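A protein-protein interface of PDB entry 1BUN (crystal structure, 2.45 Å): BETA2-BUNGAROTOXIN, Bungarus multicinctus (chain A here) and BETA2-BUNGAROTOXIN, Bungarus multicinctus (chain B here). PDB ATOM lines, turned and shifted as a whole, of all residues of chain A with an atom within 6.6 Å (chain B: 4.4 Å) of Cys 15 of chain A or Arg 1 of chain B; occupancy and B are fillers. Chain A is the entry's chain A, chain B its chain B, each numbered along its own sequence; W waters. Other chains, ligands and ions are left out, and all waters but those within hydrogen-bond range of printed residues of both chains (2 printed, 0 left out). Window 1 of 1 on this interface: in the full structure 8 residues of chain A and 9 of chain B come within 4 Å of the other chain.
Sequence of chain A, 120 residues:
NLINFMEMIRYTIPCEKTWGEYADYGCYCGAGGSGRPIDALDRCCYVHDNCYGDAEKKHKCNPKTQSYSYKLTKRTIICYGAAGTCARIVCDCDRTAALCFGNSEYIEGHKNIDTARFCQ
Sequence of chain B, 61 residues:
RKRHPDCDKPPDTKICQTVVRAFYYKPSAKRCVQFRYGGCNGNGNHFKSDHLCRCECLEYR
The backbone carbonyl oxygen of Thr 12 of chain A is in hydrogen-bond range of the backbone NH of Arg 1 of chain B. The side-chain sulfur (SG) of Cys 15 of chain A is in hydrogen-bond range of the guanidinium group (NE) of Arg 1 of chain B (3.7 Å). SG of Cys 15 of chain A is disulfide-bonded to SG of Cys 55 of chain B. SG of Cys 15 of chain A is in hydrogen-bond range of N of Glu 56 of chain B, at 3.7 Å.
OH of Tyr 11 of chain A is in hydrogen-bond range of N of Arg 75 of chain A, 2.8 Å away. The backbone carbonyl oxygen (O) of Cys 55 of chain B sits at hydrogen-bond distance from the guanidinium group (NH2) of Arg 1 of chain B.
Among the printed residues, pairs that only touch across the chains: Tyr 11 of chain A with Arg 1 of chain B (3.6 Å), Tyr 11 of chain A with Tyr 60 of chain B (3.3 Å), Ile 13 of chain A with Arg 1 of chain B (3.5 Å), Lys 74 of chain A with Tyr 60 of chain B (3.7 Å), Arg 75 of chain A with Arg 1 of chain B (3.1 Å), Arg 75 of chain A with Lys 2 of chain B (3.8 Å), Arg 75 of chain A with Cys 55 of chain B (3.6 Å) and Arg 75 of chain A with Tyr 60 of chain B (3.3 Å).
Of chain B, only Arg 1, Cys 55 and Glu 56 come within 4 Å of Cys 15 of chain A. Arg 1 of chain B touches just these residues of chain A: Tyr 11, Thr 12, Ile 13, Cys 15 and Arg 75. Printed residues of chain A within 4 Å of Cys 55 of chain B: Cys 15 and Arg 75. Printed residues of chain B within 4 Å of Lys 74 of chain A: Tyr 60 (3.7 Å). Of the printed residues of chain A, Tyr 60 of chain B touches Tyr 11, Lys 74 and Arg 75. Lys 17 of chain A touches none of the printed residues of chain B. Leu 52 of chain B touches none of the printed residues of chain A. The nearest residue of chain B that does not touch Cys 15 of chain A is Leu 52 of chain B (4.1 Å). The nearest residue of chain A that does not touch Arg 1 of chain B is Pro 14 of chain A (4.3 Å). The nearest printed residue of chain B that does not touch Ile 13 of chain A is Cys 55 of chain B (6.1 Å).
Printed residues of chain A that touch a printed residue of chain B: Tyr 11, Thr 12, Ile 13, Cys 15, Lys 74 and Arg 75. Hydrophobic or aromatic side chains of chain A that line the printed part of chain B: Tyr 11. Printed residues of chain B that touch a printed residue of chain A: Arg 1, Lys 2, Cys 55, Glu 56 and Tyr 60. Hydrophobic or aromatic side chains of chain B within 4 Å of the printed part of chain A: Tyr 60. Among the printed residues, 12 pairs touch across the chains.
Water W2 lies within hydrogen-bond range of the guanidinium group (NH1) of Arg 75 of chain A (2.6 Å), the guanidinium group (NE) of Arg 1 of chain B (2.7 Å), the backbone carbonyl oxygen (O) of Cys 55 of chain B (2.8 Å) and the backbone carbonyl oxygen (O) of Lys 2 of chain B (3.2 Å). Water W1 bridges the backbone NH (N) of Cys 15 of chain A (2.7 Å) and the side-chain carboxylate (OE1) of Glu 56 of chain B (2.9 Å).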
ATOM      1  N   ARG A  10     -16.341  22.483 -16.991  1.00  0.00           N
ATOM      2  CA  ARG A  10     -16.381  21.132 -17.466  1.00  0.00           C
ATOM      3  C   ARG A  10     -15.182  20.383 -16.944  1.00  0.00           C
ATOM      4  O   ARG A  10     -15.276  19.216 -16.628  1.00  0.00           O
ATOM      5  CB  ARG A  10     -16.454  21.136 -18.997  1.00  0.00           C
ATOM      6  CG  ARG A  10     -15.762  19.975 -19.711  1.00  0.00           C
ATOM      7  CD  ARG A  10     -16.642  18.736 -19.919  1.00  0.00           C
ATOM      8  NE  ARG A  10     -15.816  17.577 -20.277  1.00  0.00           N
ATOM      9  CZ  ARG A  10     -16.186  16.596 -21.099  1.00  0.00           C
ATOM     10  NH1 ARG A  10     -17.388  16.619 -21.676  1.00  0.00           N
ATOM     11  NH2 ARG A  10     -15.361  15.576 -21.325  1.00  0.00           N
ATOM     12  N   TYR A  11     -14.110  21.102 -16.679  1.00  0.00           N
ATOM     13  CA  TYR A  11     -12.876  20.493 -16.228  1.00  0.00           C
ATOM     14  C   TYR A  11     -12.662  20.401 -14.707  1.00  0.00           C
ATOM     15  O   TYR A  11     -11.742  19.698 -14.264  1.00  0.00           O
ATOM     16  CB  TYR A  11     -11.724  21.263 -16.898  1.00  0.00           C
ATOM     17  CG  TYR A  11     -10.329  20.732 -16.683  1.00  0.00           C
ATOM     18  CD1 TYR A  11      -9.869  19.629 -17.383  1.00  0.00           C
ATOM     19  CD2 TYR A  11      -9.466  21.343 -15.777  1.00  0.00           C
ATOM     20  CE1 TYR A  11      -8.606  19.149 -17.189  1.00  0.00           C
ATOM     21  CE2 TYR A  11      -8.199  20.867 -15.580  1.00  0.00           C
ATOM     22  CZ  TYR A  11      -7.781  19.769 -16.286  1.00  0.00           C
ATOM     23  OH  TYR A  11      -6.515  19.280 -16.062  1.00  0.00           O
ATOM     24  N   THR A  12     -13.490  21.057 -13.892  1.00  0.00           N
ATOM     25  CA  THR A  12     -13.248  21.013 -12.456  1.00  0.00           C
ATOM     26  C   THR A  12     -14.328  20.379 -11.617  1.00  0.00           C
ATOM     27  O   THR A  12     -14.064  20.000 -10.475  1.00  0.00           O
ATOM     28  CB  THR A  12     -12.922  22.414 -11.855  1.00  0.00           C
ATOM     29  OG1 THR A  12     -14.072  23.261 -11.917  1.00  0.00           O
ATOM     30  CG2 THR A  12     -11.806  23.065 -12.601  1.00  0.00           C
ATOM     31  N   ILE A  13     -15.553  20.361 -12.130  1.00  0.00           N
ATOM     32  CA  ILE A  13     -16.675  19.752 -11.418  1.00  0.00           C
ATOM     33  C   ILE A  13     -16.464  18.240 -11.462  1.00  0.00           C
ATOM     34  O   ILE A  13     -15.796  17.732 -12.366  1.00  0.00           O
ATOM     35  CB  ILE A  13     -18.037  20.087 -12.087  1.00  0.00           C
ATOM     36  CG1 ILE A  13     -18.116  19.494 -13.501  1.00  0.00           C
ATOM     37  CG2 ILE A  13     -18.207  21.582 -12.174  1.00  0.00           C
ATOM     38  CD1 ILE A  13     -19.459  19.631 -14.164  1.00  0.00           C
ATOM     39  N   PRO A  14     -16.965  17.503 -10.455  1.00  0.00           N
ATOM     40  CA  PRO A  14     -16.764  16.062 -10.501  1.00  0.00           C
ATOM     41  C   PRO A  14     -17.192  15.466 -11.834  1.00  0.00           C
ATOM     42  O   PRO A  14     -18.153  15.941 -12.457  1.00  0.00           O
ATOM     43  CB  PRO A  14     -17.634  15.567  -9.343  1.00  0.00           C
ATOM     44  CG  PRO A  14     -18.585  16.658  -9.095  1.00  0.00           C
ATOM     45  CD  PRO A  14     -17.734  17.862  -9.255  1.00  0.00           C
ATOM     46  N   CYS A  15     -16.465  14.427 -12.247  1.00  0.00           N
ATOM     47  CA  CYS A  15     -16.695  13.694 -13.497  1.00  0.00           C
ATOM     48  C   CYS A  15     -18.140  13.234 -13.806  1.00  0.00           C
ATOM     49  O   CYS A  15     -18.612  13.320 -14.947  1.00  0.00           O
ATOM     50  CB  CYS A  15     -15.763  12.488 -13.543  1.00  0.00           C
ATOM     51  SG  CYS A  15     -14.022  12.917 -13.791  1.00  0.00           S
ATOM     52  N   GLU A  16     -18.818  12.711 -12.792  1.00  0.00           N
ATOM     53  CA  GLU A  16     -20.182  12.228 -12.949  1.00  0.00           C
ATOM     54  C   GLU A  16     -21.227  13.339 -13.237  1.00  0.00           C
ATOM     55  O   GLU A  16     -22.304  13.053 -13.771  1.00  0.00           O
ATOM     56  CB  GLU A  16     -20.573  11.453 -11.687  1.00  0.00           C
ATOM     57  CG  GLU A  16     -21.848  10.616 -11.808  1.00  0.00           C
ATOM     58  CD  GLU A  16     -21.619   9.221 -12.399  1.00  0.00           C
ATOM     59  OE1 GLU A  16     -21.281   8.289 -11.627  1.00  0.00           O
ATOM     60  OE2 GLU A  16     -21.822   9.030 -13.621  1.00  0.00           O
ATOM     61  N   LYS A  17     -20.913  14.587 -12.873  1.00  0.00           N
ATOM     62  CA  LYS A  17     -21.833  15.724 -13.051  1.00  0.00           C
ATOM     63  C   LYS A  17     -21.746  16.365 -14.424  1.00  0.00           C
ATOM     64  O   LYS A  17     -20.938  15.968 -15.249  1.00  0.00           O
ATOM     65  CB  LYS A  17     -21.554  16.800 -12.004  1.00  0.00           C
ATOM     66  CG  LYS A  17     -22.642  16.982 -10.986  1.00  0.00           C
ATOM     67  CD  LYS A  17     -22.268  16.338  -9.675  1.00  0.00           C
ATOM     68  CE  LYS A  17     -23.510  15.791  -8.977  1.00  0.00           C
ATOM     69  NZ  LYS A  17     -24.634  16.769  -8.848  1.00  0.00           N
ATOM     70  N   THR A  18     -22.572  17.373 -14.666  1.00  0.00           N
ATOM     71  CA  THR A  18     -22.552  18.076 -15.941  1.00  0.00           C
ATOM     72  C   THR A  18     -22.851  19.579 -15.757  1.00  0.00           C
ATOM     73  O   THR A  18     -23.334  20.012 -14.700  1.00  0.00           O
ATOM     74  CB  THR A  18     -23.552  17.459 -16.943  1.00  0.00           C
ATOM     75  OG1 THR A  18     -24.870  17.473 -16.386  1.00  0.00           O
ATOM     76  CG2 THR A  18     -23.183  16.038 -17.267  1.00  0.00           C
ATOM     77  N   LYS A  74      -3.036  19.303 -15.293  1.00  0.00           N
ATOM     78  CA  LYS A  74      -2.886  18.795 -13.924  1.00  0.00           C
ATOM     79  C   LYS A  74      -4.116  19.026 -13.048  1.00  0.00           C
ATOM     80  O   LYS A  74      -4.000  19.343 -11.868  1.00  0.00           O
ATOM     81  CB  LYS A  74      -1.652  19.410 -13.240  1.00  0.00           C
ATOM     82  CG  LYS A  74      -0.292  18.969 -13.790  1.00  0.00           C
ATOM     83  CD  LYS A  74       0.035  19.633 -15.124  1.00  0.00           C
ATOM     84  CE  LYS A  74       1.406  19.207 -15.656  1.00  0.00           C
ATOM     85  NZ  LYS A  74       1.639  19.732 -17.036  1.00  0.00           N
ATOM     86  N   ARG A  75      -5.296  18.851 -13.628  1.00  0.00           N
ATOM     87  CA  ARG A  75      -6.548  19.048 -12.906  1.00  0.00           C
ATOM     88  C   ARG A  75      -6.741  20.480 -12.389  1.00  0.00           C
ATOM     89  O   ARG A  75      -7.622  20.734 -11.564  1.00  0.00           O
ATOM     90  CB  ARG A  75      -6.665  18.031 -11.763  1.00  0.00           C
ATOM     91  CG  ARG A  75      -7.955  17.199 -11.802  1.00  0.00           C
ATOM     92  CD  ARG A  75      -7.777  15.842 -11.128  1.00  0.00           C
ATOM     93  NE  ARG A  75      -6.690  15.096 -11.748  1.00  0.00           N
ATOM     94  CZ  ARG A  75      -6.829  13.919 -12.344  1.00  0.00           C
ATOM     95  NH1 ARG A  75      -8.019  13.329 -12.402  1.00  0.00           N
ATOM     96  NH2 ARG A  75      -5.768  13.338 -12.892  1.00  0.00           N
ATOM     97  N   THR A  76      -5.925  21.409 -12.894  1.00  0.00           N
ATOM     98  CA  THR A  76      -6.001  22.819 -12.514  1.00  0.00           C
ATOM     99  C   THR A  76      -6.134  23.720 -13.745  1.00  0.00           C
ATOM    100  O   THR A  76      -6.220  23.243 -14.885  1.00  0.00           O
ATOM    101  CB  THR A  76      -4.771  23.282 -11.705  1.00  0.00           C
ATOM    102  OG1 THR A  76      -3.625  23.327 -12.559  1.00  0.00           O
ATOM    103  CG2 THR A  76      -4.504  22.347 -10.544  1.00  0.00           C
ATOM    104  N   GLY A 102     -15.467  23.203  -8.293  1.00  0.00           N
ATOM    105  CA  GLY A 102     -14.978  21.864  -8.041  1.00  0.00           C
ATOM    106  C   GLY A 102     -14.823  21.525  -6.572  1.00  0.00           C
ATOM    107  O   GLY A 102     -15.033  20.380  -6.179  1.00  0.00           O
ATOM    108  N   ASN A 103     -14.485  22.518  -5.756  1.00  0.00           N
ATOM    109  CA  ASN A 103     -14.272  22.275  -4.342  1.00  0.00           C
ATOM    110  C   ASN A 103     -15.487  22.470  -3.469  1.00  0.00           C
ATOM    111  O   ASN A 103     -15.393  22.351  -2.247  1.00  0.00           O
ATOM    112  CB  ASN A 103     -13.115  23.123  -3.825  1.00  0.00           C
ATOM    113  CG  ASN A 103     -11.822  22.839  -4.559  1.00  0.00           C
ATOM    114  OD1 ASN A 103     -11.594  21.725  -5.045  1.00  0.00           O
ATOM    115  ND2 ASN A 103     -10.987  23.856  -4.695  1.00  0.00           N
ATOM    116  N   ARG B   1     -11.656  19.162  -9.554  1.00  0.00           N
ATOM    117  CA  ARG B   1     -11.859  17.733  -9.188  1.00  0.00           C
ATOM    118  C   ARG B   1     -10.522  17.091  -8.824  1.00  0.00           C
ATOM    119  O   ARG B   1      -9.461  17.600  -9.179  1.00  0.00           O
ATOM    120  CB  ARG B   1     -12.548  16.967 -10.335  1.00  0.00           C
ATOM    121  CG  ARG B   1     -11.962  17.230 -11.700  1.00  0.00           C
ATOM    122  CD  ARG B   1     -12.580  16.379 -12.780  1.00  0.00           C
ATOM    123  NE  ARG B   1     -11.532  15.641 -13.479  1.00  0.00           N
ATOM    124  CZ  ARG B   1     -11.305  15.675 -14.789  1.00  0.00           C
ATOM    125  NH1 ARG B   1     -12.071  16.413 -15.592  1.00  0.00           N
ATOM    126  NH2 ARG B   1     -10.278  14.982 -15.285  1.00  0.00           N
ATOM    127  N   LYS B   2     -10.584  15.994  -8.077  1.00  0.00           N
ATOM    128  CA  LYS B   2      -9.391  15.275  -7.662  1.00  0.00           C
ATOM    129  C   LYS B   2      -9.397  13.895  -8.295  1.00  0.00           C
ATOM    130  O   LYS B   2     -10.429  13.442  -8.808  1.00  0.00           O
ATOM    131  CB  LYS B   2      -9.344  15.169  -6.136  1.00  0.00           C
ATOM    132  CG  LYS B   2      -9.075  16.502  -5.457  1.00  0.00           C
ATOM    133  CD  LYS B   2      -9.233  16.464  -3.938  1.00  0.00           C
ATOM    134  CE  LYS B   2     -10.682  16.570  -3.474  1.00  0.00           C
ATOM    135  NZ  LYS B   2     -11.392  15.273  -3.607  1.00  0.00           N
ATOM    136  N   LEU B  52     -15.560   7.971 -18.484  1.00  0.00           N
ATOM    137  CA  LEU B  52     -15.706   8.206 -17.048  1.00  0.00           C
ATOM    138  C   LEU B  52     -14.424   7.770 -16.295  1.00  0.00           C
ATOM    139  O   LEU B  52     -13.929   8.449 -15.370  1.00  0.00           O
ATOM    140  CB  LEU B  52     -16.909   7.402 -16.539  1.00  0.00           C
ATOM    141  CG  LEU B  52     -17.190   7.571 -15.051  1.00  0.00           C
ATOM    142  CD1 LEU B  52     -17.581   9.020 -14.788  1.00  0.00           C
ATOM    143  CD2 LEU B  52     -18.256   6.596 -14.553  1.00  0.00           C
ATOM    144  N   CYS B  55     -11.446  10.085 -17.116  1.00  0.00           N
ATOM    145  CA  CYS B  55     -11.817  11.269 -16.364  1.00  0.00           C
ATOM    146  C   CYS B  55     -11.396  11.196 -14.911  1.00  0.00           C
ATOM    147  O   CYS B  55     -10.833  12.149 -14.376  1.00  0.00           O
ATOM    148  CB  CYS B  55     -13.326  11.438 -16.410  1.00  0.00           C
ATOM    149  SG  CYS B  55     -13.873  13.052 -15.804  1.00  0.00           S
ATOM    150  N   GLU B  56     -11.670  10.053 -14.287  1.00  0.00           N
ATOM    151  CA  GLU B  56     -11.385   9.840 -12.879  1.00  0.00           C
ATOM    152  C   GLU B  56      -9.976   9.407 -12.542  1.00  0.00           C
ATOM    153  O   GLU B  56      -9.508   9.672 -11.429  1.00  0.00           O
ATOM    154  CB  GLU B  56     -12.337   8.782 -12.302  1.00  0.00           C
ATOM    155  CG  GLU B  56     -13.780   9.166 -12.183  1.00  0.00           C
ATOM    156  CD  GLU B  56     -14.111   9.756 -10.836  1.00  0.00           C
ATOM    157  OE1 GLU B  56     -13.413  10.689 -10.393  1.00  0.00           O
ATOM    158  OE2 GLU B  56     -15.091   9.305 -10.221  1.00  0.00           O
ATOM    159  N   TYR B  60      -2.119  13.048 -15.041  1.00  0.00           N
ATOM    160  CA  TYR B  60      -1.642  14.198 -15.793  1.00  0.00           C
ATOM    161  C   TYR B  60      -0.133  14.389 -15.653  1.00  0.00           C
ATOM    162  O   TYR B  60       0.331  15.367 -15.060  1.00  0.00           O
ATOM    163  CB  TYR B  60      -2.406  15.465 -15.377  1.00  0.00           C
ATOM    164  CG  TYR B  60      -3.824  15.533 -15.923  1.00  0.00           C
ATOM    165  CD1 TYR B  60      -4.087  15.230 -17.251  1.00  0.00           C
ATOM    166  CD2 TYR B  60      -4.888  15.922 -15.120  1.00  0.00           C
ATOM    167  CE1 TYR B  60      -5.367  15.314 -17.768  1.00  0.00           C
ATOM    168  CE2 TYR B  60      -6.175  16.009 -15.632  1.00  0.00           C
ATOM    169  CZ  TYR B  60      -6.404  15.704 -16.961  1.00  0.00           C
ATOM    170  OH  TYR B  60      -7.670  15.793 -17.494  1.00  0.00           O
HETATM  171  O   HOH W   1     -15.164  13.061 -10.298  1.00  0.00           O
HETATM  172  O   HOH W   2     -10.587  13.599 -12.004  1.00  0.00           O
